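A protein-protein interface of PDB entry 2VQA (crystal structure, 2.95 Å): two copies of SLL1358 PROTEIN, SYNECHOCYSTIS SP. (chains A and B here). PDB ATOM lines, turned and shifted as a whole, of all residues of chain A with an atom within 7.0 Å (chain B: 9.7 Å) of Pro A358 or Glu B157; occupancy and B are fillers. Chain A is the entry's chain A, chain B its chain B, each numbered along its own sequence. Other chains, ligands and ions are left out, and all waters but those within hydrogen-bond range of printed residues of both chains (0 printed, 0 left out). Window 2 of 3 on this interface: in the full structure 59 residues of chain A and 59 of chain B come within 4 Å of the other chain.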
ATOM      1  N   ASN A 218       4.555  15.588   8.111  1.00  0.00           N
ATOM      2  CA  ASN A 218       5.643  14.966   7.365  1.00  0.00           C
ATOM      3  C   ASN A 218       6.483  14.005   8.218  1.00  0.00           C
ATOM      4  O   ASN A 218       6.829  14.316   9.359  1.00  0.00           O
ATOM      5  CB  ASN A 218       6.481  16.046   6.720  1.00  0.00           C
ATOM      6  CG  ASN A 218       5.644  16.963   5.887  1.00  0.00           C
ATOM      7  OD1 ASN A 218       5.237  16.604   4.786  1.00  0.00           O
ATOM      8  ND2 ASN A 218       5.348  18.144   6.412  1.00  0.00           N
ATOM      9  N   GLU A 242       3.130  15.727   3.225  1.00  0.00           N
ATOM     10  CA  GLU A 242       1.894  16.495   3.161  1.00  0.00           C
ATOM     11  C   GLU A 242       1.875  17.385   1.914  1.00  0.00           C
ATOM     12  O   GLU A 242       2.942  17.708   1.373  1.00  0.00           O
ATOM     13  CB  GLU A 242       1.776  17.363   4.404  1.00  0.00           C
ATOM     14  CG  GLU A 242       1.485  16.588   5.650  1.00  0.00           C
ATOM     15  CD  GLU A 242       0.299  15.666   5.465  1.00  0.00           C
ATOM     16  OE1 GLU A 242      -0.631  16.019   4.699  1.00  0.00           O
ATOM     17  OE2 GLU A 242       0.295  14.575   6.082  1.00  0.00           O
ATOM     18  N   PRO A 243       0.671  17.776   1.433  1.00  0.00           N
ATOM     19  CA  PRO A 243       0.658  18.663   0.248  1.00  0.00           C
ATOM     20  C   PRO A 243       1.473  19.942   0.466  1.00  0.00           C
ATOM     21  O   PRO A 243       1.351  20.584   1.504  1.00  0.00           O
ATOM     22  CB  PRO A 243      -0.827  18.984   0.067  1.00  0.00           C
ATOM     23  CG  PRO A 243      -1.543  17.806   0.708  1.00  0.00           C
ATOM     24  CD  PRO A 243      -0.689  17.428   1.889  1.00  0.00           C
ATOM     25  N   GLY A 244       2.338  20.286  -0.482  1.00  0.00           N
ATOM     26  CA  GLY A 244       3.099  21.536  -0.383  1.00  0.00           C
ATOM     27  C   GLY A 244       4.474  21.440   0.265  1.00  0.00           C
ATOM     28  O   GLY A 244       5.315  22.335   0.103  1.00  0.00           O
ATOM     29  N   ALA A 245       4.710  20.344   0.981  1.00  0.00           N
ATOM     30  CA  ALA A 245       5.934  20.163   1.752  1.00  0.00           C
ATOM     31  C   ALA A 245       7.064  19.556   0.922  1.00  0.00           C
ATOM     32  O   ALA A 245       6.833  18.996  -0.151  1.00  0.00           O
ATOM     33  CB  ALA A 245       5.642  19.282   2.972  1.00  0.00           C
ATOM     34  N   MET A 246       8.290  19.651   1.425  1.00  0.00           N
ATOM     35  CA  MET A 246       9.406  19.008   0.748  1.00  0.00           C
ATOM     36  C   MET A 246      10.420  18.403   1.731  1.00  0.00           C
ATOM     37  O   MET A 246      10.472  18.797   2.902  1.00  0.00           O
ATOM     38  CB  MET A 246      10.083  19.997  -0.198  1.00  0.00           C
ATOM     39  CG  MET A 246      10.485  21.301   0.466  1.00  0.00           C
ATOM     40  SD  MET A 246      11.326  22.462  -0.644  1.00  0.00           S
ATOM     41  CE  MET A 246      12.970  21.749  -0.767  1.00  0.00           C
ATOM     42  N   GLN A 248      14.157  18.604   2.478  1.00  0.00           N
ATOM     43  CA  GLN A 248      15.065  19.707   2.171  1.00  0.00           C
ATOM     44  C   GLN A 248      16.149  19.279   1.197  1.00  0.00           C
ATOM     45  O   GLN A 248      16.350  18.086   0.978  1.00  0.00           O
ATOM     46  CB  GLN A 248      15.696  20.239   3.436  1.00  0.00           C
ATOM     47  CG  GLN A 248      14.722  20.920   4.329  1.00  0.00           C
ATOM     48  CD  GLN A 248      15.412  21.612   5.477  1.00  0.00           C
ATOM     49  OE1 GLN A 248      16.637  21.786   5.468  1.00  0.00           O
ATOM     50  NE2 GLN A 248      14.634  22.013   6.479  1.00  0.00           N
ATOM     51  N   ARG A 299       9.608  17.295  -3.575  1.00  0.00           N
ATOM     52  CA  ARG A 299       8.469  18.127  -3.182  1.00  0.00           C
ATOM     53  C   ARG A 299       7.151  17.519  -3.650  1.00  0.00           C
ATOM     54  O   ARG A 299       7.046  17.015  -4.777  1.00  0.00           O
ATOM     55  CB  ARG A 299       8.621  19.524  -3.786  1.00  0.00           C
ATOM     56  CG  ARG A 299       7.528  20.505  -3.440  1.00  0.00           C
ATOM     57  CD  ARG A 299       7.897  21.931  -3.877  1.00  0.00           C
ATOM     58  NE  ARG A 299       7.141  22.895  -3.081  1.00  0.00           N
ATOM     59  CZ  ARG A 299       5.912  23.335  -3.374  1.00  0.00           C
ATOM     60  NH1 ARG A 299       5.282  22.924  -4.473  1.00  0.00           N
ATOM     61  NH2 ARG A 299       5.307  24.188  -2.552  1.00  0.00           N
ATOM     62  N   ASN A 300       6.162  17.572  -2.762  1.00  0.00           N
ATOM     63  CA  ASN A 300       4.775  17.220  -3.062  1.00  0.00           C
ATOM     64  C   ASN A 300       4.030  18.468  -3.545  1.00  0.00           C
ATOM     65  O   ASN A 300       3.730  19.376  -2.761  1.00  0.00           O
ATOM     66  CB  ASN A 300       4.118  16.619  -1.809  1.00  0.00           C
ATOM     67  CG  ASN A 300       2.633  16.313  -1.990  1.00  0.00           C
ATOM     68  OD1 ASN A 300       2.035  16.635  -3.014  1.00  0.00           O
ATOM     69  ND2 ASN A 300       2.028  15.688  -0.974  1.00  0.00           N
ATOM     70  N   PHE A 355      12.361  18.352   6.786  1.00  0.00           N
ATOM     71  CA  PHE A 355      11.332  18.784   5.855  1.00  0.00           C
ATOM     72  C   PHE A 355      11.185  20.291   5.918  1.00  0.00           C
ATOM     73  O   PHE A 355      11.622  20.915   6.888  1.00  0.00           O
ATOM     74  CB  PHE A 355      10.003  18.142   6.206  1.00  0.00           C
ATOM     75  CG  PHE A 355      10.042  16.658   6.192  1.00  0.00           C
ATOM     76  CD1 PHE A 355      10.084  15.963   4.986  1.00  0.00           C
ATOM     77  CD2 PHE A 355      10.052  15.941   7.378  1.00  0.00           C
ATOM     78  CE1 PHE A 355      10.134  14.571   4.973  1.00  0.00           C
ATOM     79  CE2 PHE A 355      10.095  14.552   7.369  1.00  0.00           C
ATOM     80  CZ  PHE A 355      10.140  13.868   6.168  1.00  0.00           C
ATOM     81  N   SER A 356      10.577  20.873   4.886  1.00  0.00           N
ATOM     82  CA  SER A 356      10.248  22.296   4.881  1.00  0.00           C
ATOM     83  C   SER A 356       8.771  22.452   4.563  1.00  0.00           C
ATOM     84  O   SER A 356       8.233  21.735   3.704  1.00  0.00           O
ATOM     85  CB  SER A 356      11.093  23.043   3.857  1.00  0.00           C
ATOM     86  OG  SER A 356      12.362  23.374   4.387  1.00  0.00           O
ATOM     87  N   LEU A 357       8.109  23.375   5.262  1.00  0.00           N
ATOM     88  CA  LEU A 357       6.643  23.511   5.176  1.00  0.00           C
ATOM     89  C   LEU A 357       6.228  24.569   4.172  1.00  0.00           C
ATOM     90  O   LEU A 357       6.984  25.504   3.909  1.00  0.00           O
ATOM     91  CB  LEU A 357       6.063  23.850   6.543  1.00  0.00           C
ATOM     92  CG  LEU A 357       6.552  22.896   7.630  1.00  0.00           C
ATOM     93  CD1 LEU A 357       6.049  23.296   9.017  1.00  0.00           C
ATOM     94  CD2 LEU A 357       6.165  21.458   7.271  1.00  0.00           C
ATOM     95  N   PRO A 358       5.020  24.426   3.585  1.00  0.00           N
ATOM     96  CA  PRO A 358       4.551  25.538   2.743  1.00  0.00           C
ATOM     97  C   PRO A 358       4.167  26.675   3.691  1.00  0.00           C
ATOM     98  O   PRO A 358       3.920  26.427   4.890  1.00  0.00           O
ATOM     99  CB  PRO A 358       3.336  24.957   2.035  1.00  0.00           C
ATOM    100  CG  PRO A 358       2.871  23.835   2.936  1.00  0.00           C
ATOM    101  CD  PRO A 358       4.052  23.314   3.665  1.00  0.00           C
ATOM    102  N   THR A 359       4.146  27.912   3.212  1.00  0.00           N
ATOM    103  CA  THR A 359       3.946  29.012   4.164  1.00  0.00           C
ATOM    104  C   THR A 359       2.605  28.904   4.917  1.00  0.00           C
ATOM    105  O   THR A 359       1.570  28.511   4.340  1.00  0.00           O
ATOM    106  CB  THR A 359       4.067  30.410   3.509  1.00  0.00           C
ATOM    107  OG1 THR A 359       2.864  30.684   2.787  1.00  0.00           O
ATOM    108  CG2 THR A 359       5.327  30.492   2.587  1.00  0.00           C
ATOM    109  N   GLN A 360       2.656  29.256   6.208  1.00  0.00           N
ATOM    110  CA  GLN A 360       1.505  29.178   7.156  1.00  0.00           C
ATOM    111  C   GLN A 360       0.429  30.246   6.978  1.00  0.00           C
ATOM    112  O   GLN A 360       0.730  31.392   6.624  1.00  0.00           O
ATOM    113  CB  GLN A 360       2.000  29.297   8.617  1.00  0.00           C
ATOM    114  CG  GLN A 360       3.227  28.457   8.938  1.00  0.00           C
ATOM    115  CD  GLN A 360       3.081  27.013   8.439  1.00  0.00           C
ATOM    116  OE1 GLN A 360       1.946  26.500   8.253  1.00  0.00           O
ATOM    117  NE2 GLN A 360       4.220  26.349   8.219  1.00  0.00           N
ATOM    118  N   PRO A 361      -0.829  29.877   7.283  1.00  0.00           N
ATOM    119  CA  PRO A 361      -2.020  30.802   7.417  1.00  0.00           C
ATOM    120  C   PRO A 361      -1.780  32.086   8.282  1.00  0.00           C
ATOM    121  O   PRO A 361      -0.947  32.094   9.220  1.00  0.00           O
ATOM    122  CB  PRO A 361      -3.111  29.915   8.071  1.00  0.00           C
ATOM    123  CG  PRO A 361      -2.386  28.524   8.441  1.00  0.00           C
ATOM    124  CD  PRO A 361      -1.153  28.448   7.523  1.00  0.00           C
ATOM    125  N   THR B 150      18.250  24.904  -8.932  1.00  0.00           N
ATOM    126  CA  THR B 150      17.144  24.242  -8.255  1.00  0.00           C
ATOM    127  C   THR B 150      15.946  25.141  -8.522  1.00  0.00           C
ATOM    128  O   THR B 150      16.118  26.344  -8.638  1.00  0.00           O
ATOM    129  CB  THR B 150      17.418  24.182  -6.735  1.00  0.00           C
ATOM    130  OG1 THR B 150      18.581  23.390  -6.481  1.00  0.00           O
ATOM    131  CG2 THR B 150      16.256  23.581  -5.980  1.00  0.00           C
ATOM    132  N   PRO B 151      14.731  24.580  -8.648  1.00  0.00           N
ATOM    133  CA  PRO B 151      13.578  25.451  -8.804  1.00  0.00           C
ATOM    134  C   PRO B 151      13.536  26.533  -7.743  1.00  0.00           C
ATOM    135  O   PRO B 151      13.562  26.227  -6.547  1.00  0.00           O
ATOM    136  CB  PRO B 151      12.396  24.495  -8.604  1.00  0.00           C
ATOM    137  CG  PRO B 151      12.878  23.206  -9.122  1.00  0.00           C
ATOM    138  CD  PRO B 151      14.335  23.159  -8.678  1.00  0.00           C
ATOM    139  N   ILE B 152      13.466  27.783  -8.196  1.00  0.00           N
ATOM    140  CA  ILE B 152      13.363  28.953  -7.318  1.00  0.00           C
ATOM    141  C   ILE B 152      12.334  28.808  -6.167  1.00  0.00           C
ATOM    142  O   ILE B 152      12.679  29.021  -5.004  1.00  0.00           O
ATOM    143  CB  ILE B 152      13.110  30.253  -8.140  1.00  0.00           C
ATOM    144  CG1 ILE B 152      14.354  30.624  -8.948  1.00  0.00           C
ATOM    145  CG2 ILE B 152      12.780  31.416  -7.235  1.00  0.00           C
ATOM    146  CD1 ILE B 152      14.309  32.016  -9.553  1.00  0.00           C
ATOM    147  N   ALA B 153      11.095  28.422  -6.471  1.00  0.00           N
ATOM    148  CA  ALA B 153      10.095  28.199  -5.412  1.00  0.00           C
ATOM    149  C   ALA B 153      10.587  27.251  -4.305  1.00  0.00           C
ATOM    150  O   ALA B 153      10.229  27.414  -3.139  1.00  0.00           O
ATOM    151  CB  ALA B 153       8.780  27.683  -6.014  1.00  0.00           C
ATOM    152  N   TRP B 154      11.397  26.254  -4.680  1.00  0.00           N
ATOM    153  CA  TRP B 154      11.932  25.278  -3.710  1.00  0.00           C
ATOM    154  C   TRP B 154      13.066  25.909  -2.912  1.00  0.00           C
ATOM    155  O   TRP B 154      13.202  25.651  -1.716  1.00  0.00           O
ATOM    156  CB  TRP B 154      12.411  23.973  -4.373  1.00  0.00           C
ATOM    157  CG  TRP B 154      11.385  23.241  -5.236  1.00  0.00           C
ATOM    158  CD1 TRP B 154      10.286  23.779  -5.840  1.00  0.00           C
ATOM    159  CD2 TRP B 154      11.410  21.856  -5.629  1.00  0.00           C
ATOM    160  NE1 TRP B 154       9.622  22.817  -6.567  1.00  0.00           N
ATOM    161  CE2 TRP B 154      10.289  21.631  -6.452  1.00  0.00           C
ATOM    162  CE3 TRP B 154      12.264  20.787  -5.358  1.00  0.00           C
ATOM    163  CZ2 TRP B 154       9.999  20.383  -7.002  1.00  0.00           C
ATOM    164  CZ3 TRP B 154      11.967  19.536  -5.913  1.00  0.00           C
ATOM    165  CH2 TRP B 154      10.847  19.351  -6.726  1.00  0.00           C
ATOM    166  N   VAL B 155      13.878  26.741  -3.550  1.00  0.00           N
ATOM    167  CA  VAL B 155      14.881  27.435  -2.778  1.00  0.00           C
ATOM    168  C   VAL B 155      14.195  28.354  -1.778  1.00  0.00           C
ATOM    169  O   VAL B 155      14.643  28.486  -0.635  1.00  0.00           O
ATOM    170  CB  VAL B 155      15.878  28.202  -3.642  1.00  0.00           C
ATOM    171  CG1 VAL B 155      16.851  28.941  -2.759  1.00  0.00           C
ATOM    172  CG2 VAL B 155      16.640  27.235  -4.541  1.00  0.00           C
ATOM    173  N   GLU B 156      13.095  28.970  -2.202  1.00  0.00           N
ATOM    174  CA  GLU B 156      12.321  29.851  -1.314  1.00  0.00           C
ATOM    175  C   GLU B 156      11.845  29.085  -0.072  1.00  0.00           C
ATOM    176  O   GLU B 156      12.081  29.510   1.071  1.00  0.00           O
ATOM    177  CB  GLU B 156      11.110  30.482  -2.032  1.00  0.00           C
ATOM    178  CG  GLU B 156      11.407  31.067  -3.424  1.00  0.00           C
ATOM    179  CD  GLU B 156      10.372  32.103  -3.890  1.00  0.00           C
ATOM    180  OE1 GLU B 156       9.764  32.773  -3.021  1.00  0.00           O
ATOM    181  OE2 GLU B 156      10.181  32.272  -5.120  1.00  0.00           O
ATOM    182  N   GLU B 157      11.173  27.961  -0.309  1.00  0.00           N
ATOM    183  CA  GLU B 157      10.626  27.127   0.765  1.00  0.00           C
ATOM    184  C   GLU B 157      11.726  26.557   1.674  1.00  0.00           C
ATOM    185  O   GLU B 157      11.581  26.508   2.895  1.00  0.00           O
ATOM    186  CB  GLU B 157       9.810  25.986   0.154  1.00  0.00           C
ATOM    187  CG  GLU B 157       9.046  25.155   1.151  1.00  0.00           C
ATOM    188  CD  GLU B 157       8.135  24.135   0.480  1.00  0.00           C
ATOM    189  OE1 GLU B 157       8.120  24.075  -0.766  1.00  0.00           O
ATOM    190  OE2 GLU B 157       7.429  23.380   1.198  1.00  0.00           O
ATOM    191  N   ASN B 158      12.826  26.118   1.076  1.00  0.00           N
ATOM    192  CA  ASN B 158      13.895  25.538   1.852  1.00  0.00           C
ATOM    193  C   ASN B 158      14.516  26.581   2.782  1.00  0.00           C
ATOM    194  O   ASN B 158      14.916  26.280   3.895  1.00  0.00           O
ATOM    195  CB  ASN B 158      14.950  24.922   0.929  1.00  0.00           C
ATOM    196  CG  ASN B 158      15.719  23.793   1.588  1.00  0.00           C
ATOM    197  OD1 ASN B 158      15.918  22.731   0.994  1.00  0.00           O
ATOM    198  ND2 ASN B 158      16.144  24.010   2.815  1.00  0.00           N
ATOM    199  N   LEU B 159      14.595  27.818   2.338  1.00  0.00           N
ATOM    200  CA  LEU B 159      15.292  28.804   3.124  1.00  0.00           C
ATOM    201  C   LEU B 159      14.341  29.673   3.909  1.00  0.00           C
ATOM    202  O   LEU B 159      14.781  30.479   4.702  1.00  0.00           O
ATOM    203  CB  LEU B 159      16.138  29.685   2.214  1.00  0.00           C
ATOM    204  CG  LEU B 159      17.261  28.959   1.496  1.00  0.00           C
ATOM    205  CD1 LEU B 159      17.977  29.972   0.635  1.00  0.00           C
ATOM    206  CD2 LEU B 159      18.201  28.364   2.507  1.00  0.00           C
ATOM    207  N   GLY B 160      13.043  29.530   3.677  1.00  0.00           N
ATOM    208  CA  GLY B 160      12.072  30.467   4.236  1.00  0.00           C
ATOM    209  C   GLY B 160      12.401  31.893   3.819  1.00  0.00           C
ATOM    210  O   GLY B 160      12.583  32.754   4.666  1.00  0.00           O
ATOM    211  N   TRP B 161      12.482  32.125   2.507  1.00  0.00           N
ATOM    212  CA  TRP B 161      12.933  33.394   1.924  1.00  0.00           C
ATOM    213  C   TRP B 161      11.972  33.831   0.822  1.00  0.00           C
ATOM    214  O   TRP B 161      11.312  32.995   0.180  1.00  0.00           O
ATOM    215  CB  TRP B 161      14.301  33.214   1.261  1.00  0.00           C
ATOM    216  CG  TRP B 161      15.513  33.338   2.139  1.00  0.00           C
ATOM    217  CD1 TRP B 161      15.579  33.136   3.483  1.00  0.00           C
ATOM    218  CD2 TRP B 161      16.848  33.657   1.712  1.00  0.00           C
ATOM    219  NE1 TRP B 161      16.865  33.331   3.928  1.00  0.00           N
ATOM    220  CE2 TRP B 161      17.668  33.648   2.862  1.00  0.00           C
ATOM    221  CE3 TRP B 161      17.426  33.963   0.472  1.00  0.00           C
ATOM    222  CZ2 TRP B 161      19.042  33.929   2.812  1.00  0.00           C
ATOM    223  CZ3 TRP B 161      18.795  34.239   0.421  1.00  0.00           C
ATOM    224  CH2 TRP B 161      19.583  34.223   1.586  1.00  0.00           C
ATOM    225  N   THR B 162      11.919  35.136   0.569  1.00  0.00           N
ATOM    226  CA  THR B 162      11.057  35.653  -0.490  1.00  0.00           C
ATOM    227  C   THR B 162      11.771  35.525  -1.833  1.00  0.00           C
ATOM    228  O   THR B 162      13.006  35.350  -1.880  1.00  0.00           O
ATOM    229  CB  THR B 162      10.692  37.129  -0.255  1.00  0.00           C
ATOM    230  OG1 THR B 162      11.791  37.974  -0.648  1.00  0.00           O
ATOM    231  CG2 THR B 162      10.367  37.363   1.208  1.00  0.00           C
ATOM    232  N   ALA B 163      11.007  35.614  -2.922  1.00  0.00           N
ATOM    233  CA  ALA B 163      11.616  35.620  -4.255  1.00  0.00           C
ATOM    234  C   ALA B 163      12.631  36.772  -4.359  1.00  0.00           C
ATOM    235  O   ALA B 163      13.745  36.593  -4.868  1.00  0.00           O
ATOM    236  CB  ALA B 163      10.553  35.726  -5.341  1.00  0.00           C
ATOM    237  N   GLN B 165      14.456  37.895  -2.073  1.00  0.00           N
ATOM    238  CA  GLN B 165      15.681  37.491  -1.349  1.00  0.00           C
ATOM    239  C   GLN B 165      16.508  36.449  -2.112  1.00  0.00           C
ATOM    240  O   GLN B 165      17.741  36.500  -2.119  1.00  0.00           O
ATOM    241  CB  GLN B 165      15.344  36.960   0.044  1.00  0.00           C
ATOM    242  CG  GLN B 165      14.775  37.995   0.962  1.00  0.00           C
ATOM    243  CD  GLN B 165      14.421  37.432   2.314  1.00  0.00           C
ATOM    244  OE1 GLN B 165      13.509  36.607   2.447  1.00  0.00           O
ATOM    245  NE2 GLN B 165      15.136  37.884   3.339  1.00  0.00           N
ATOM    246  N   VAL B 166      15.831  35.497  -2.746  1.00  0.00           N
ATOM    247  CA  VAL B 166      16.530  34.517  -3.551  1.00  0.00           C
ATOM    248  C   VAL B 166      17.194  35.159  -4.781  1.00  0.00           C
ATOM    249  O   VAL B 166      18.251  34.718  -5.212  1.00  0.00           O
ATOM    250  CB  VAL B 166      15.594  33.378  -3.955  1.00  0.00           C
ATOM    251  CG1 VAL B 166      16.107  32.666  -5.187  1.00  0.00           C
ATOM    252  CG2 VAL B 166      15.418  32.420  -2.797  1.00  0.00           C
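The side-chain carboxylate of Glu B157 lies within salt-bridge range of the guanidinium group of Arg A299, 2.8 Å away.
O of Gly A244 lies close to OE2 of Glu B157, at 2.6 Å.
O of Leu A357 sits close to OE2 of Glu B157, at 3.5 Å.
OE1 of Gln A248 lies within hydrogen-bond range of ND2 of Asn B158, 3.5 Å away.
The side-chain carboxylate (OE1) of Glu B157 lies close to the side-chain sulfur (SD) of Met A246, 3.6 Å away.
O of Ser A356 sits close to OE2 of Glu B157 (3.1 Å).
No position is printed for both chains.
Of the 12 pairs that touch across the chains among the printed residues, none has its exchanged pair printed and touching as well.
The side-chain hydroxyl of Ser A356 sits at hydrogen-bond distance from the side-chain amide nitrogen of Gln A248 (3.4 Å).
The backbone carbonyl oxygen of Asn A300 sits at hydrogen-bond distance from the backbone NH of Gly A244.
N of Asn A300 sits at hydrogen-bond distance from O of Ala A245.
O of Pro A358 is in hydrogen-bond range of NE2 of Gln A360 (3.3 Å).
The backbone NH (N) of Ser A356 is in hydrogen-bond range of the backbone carbonyl oxygen (O) of Met A246.
The guanidinium group of Arg A299 sits at hydrogen-bond distance from the backbone carbonyl oxygen of Gly A244, at 3.2 Å.
Of chain B, only Glu B157 comes within 4 Å of Pro A358.
Glu B157 touches seven residues of chain A.
Gly A244 touches one residue of chain B.
Ala A245 touches just one residue of chain B: Glu B157.
Ser A356 touches just these residues of chain B: Glu B157 and Asn B158.
Leu A357 touches just one residue of chain B: Glu B157 (3.4 Å).
Of the printed residues of chain A, Trp B154 touches Met A246 (3.9 Å) and Arg A299 (3.3 Å).
Of the printed residues of chain B, Met A246 touches Trp B154, Glu B157 and Asn B158.
Printed residues of chain A within 4 Å of Asn B158: Met A246, Gln A248 and Ser A356.
Asn A300 touches none of the printed residues of chain B.
Gly B160 touches none of the printed residues of chain A.
The nearest printed residue of chain B that does not touch Pro A358 is Asn B158 (8.4 Å).
The nearest printed residue of chain A that does not touch Trp B154 is Asn A300 (6.4 Å).
Ala A245 touches Glu B157 (CA to OE2, 3.6 Å).
Trp B154 touches Met A246 (O to SD, 3.9 Å).
CE of Met A246 touches OD1 of Asn B158, at 3.6 Å.
CD of Arg A299 touches NE1 of Trp B154, at 3.3 Å.
Asn B158 touches Ser A356 (CA to OG, 3.7 Å).
Pro A358 touches Glu B157 (N to OE2, 3.5 Å).
Hydrophobic or aromatic side chains of chain B that line the printed part of chain A: Trp B154.
Printed residues of chain A that touch a printed residue of chain B: Gly A244, Ala A245, Met A246, Gln A248, Arg A299, Ser A356, Leu A357 and Pro A358.
Hydrophobic or aromatic side chains of chain A that line the printed part of chain B: Met A246.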
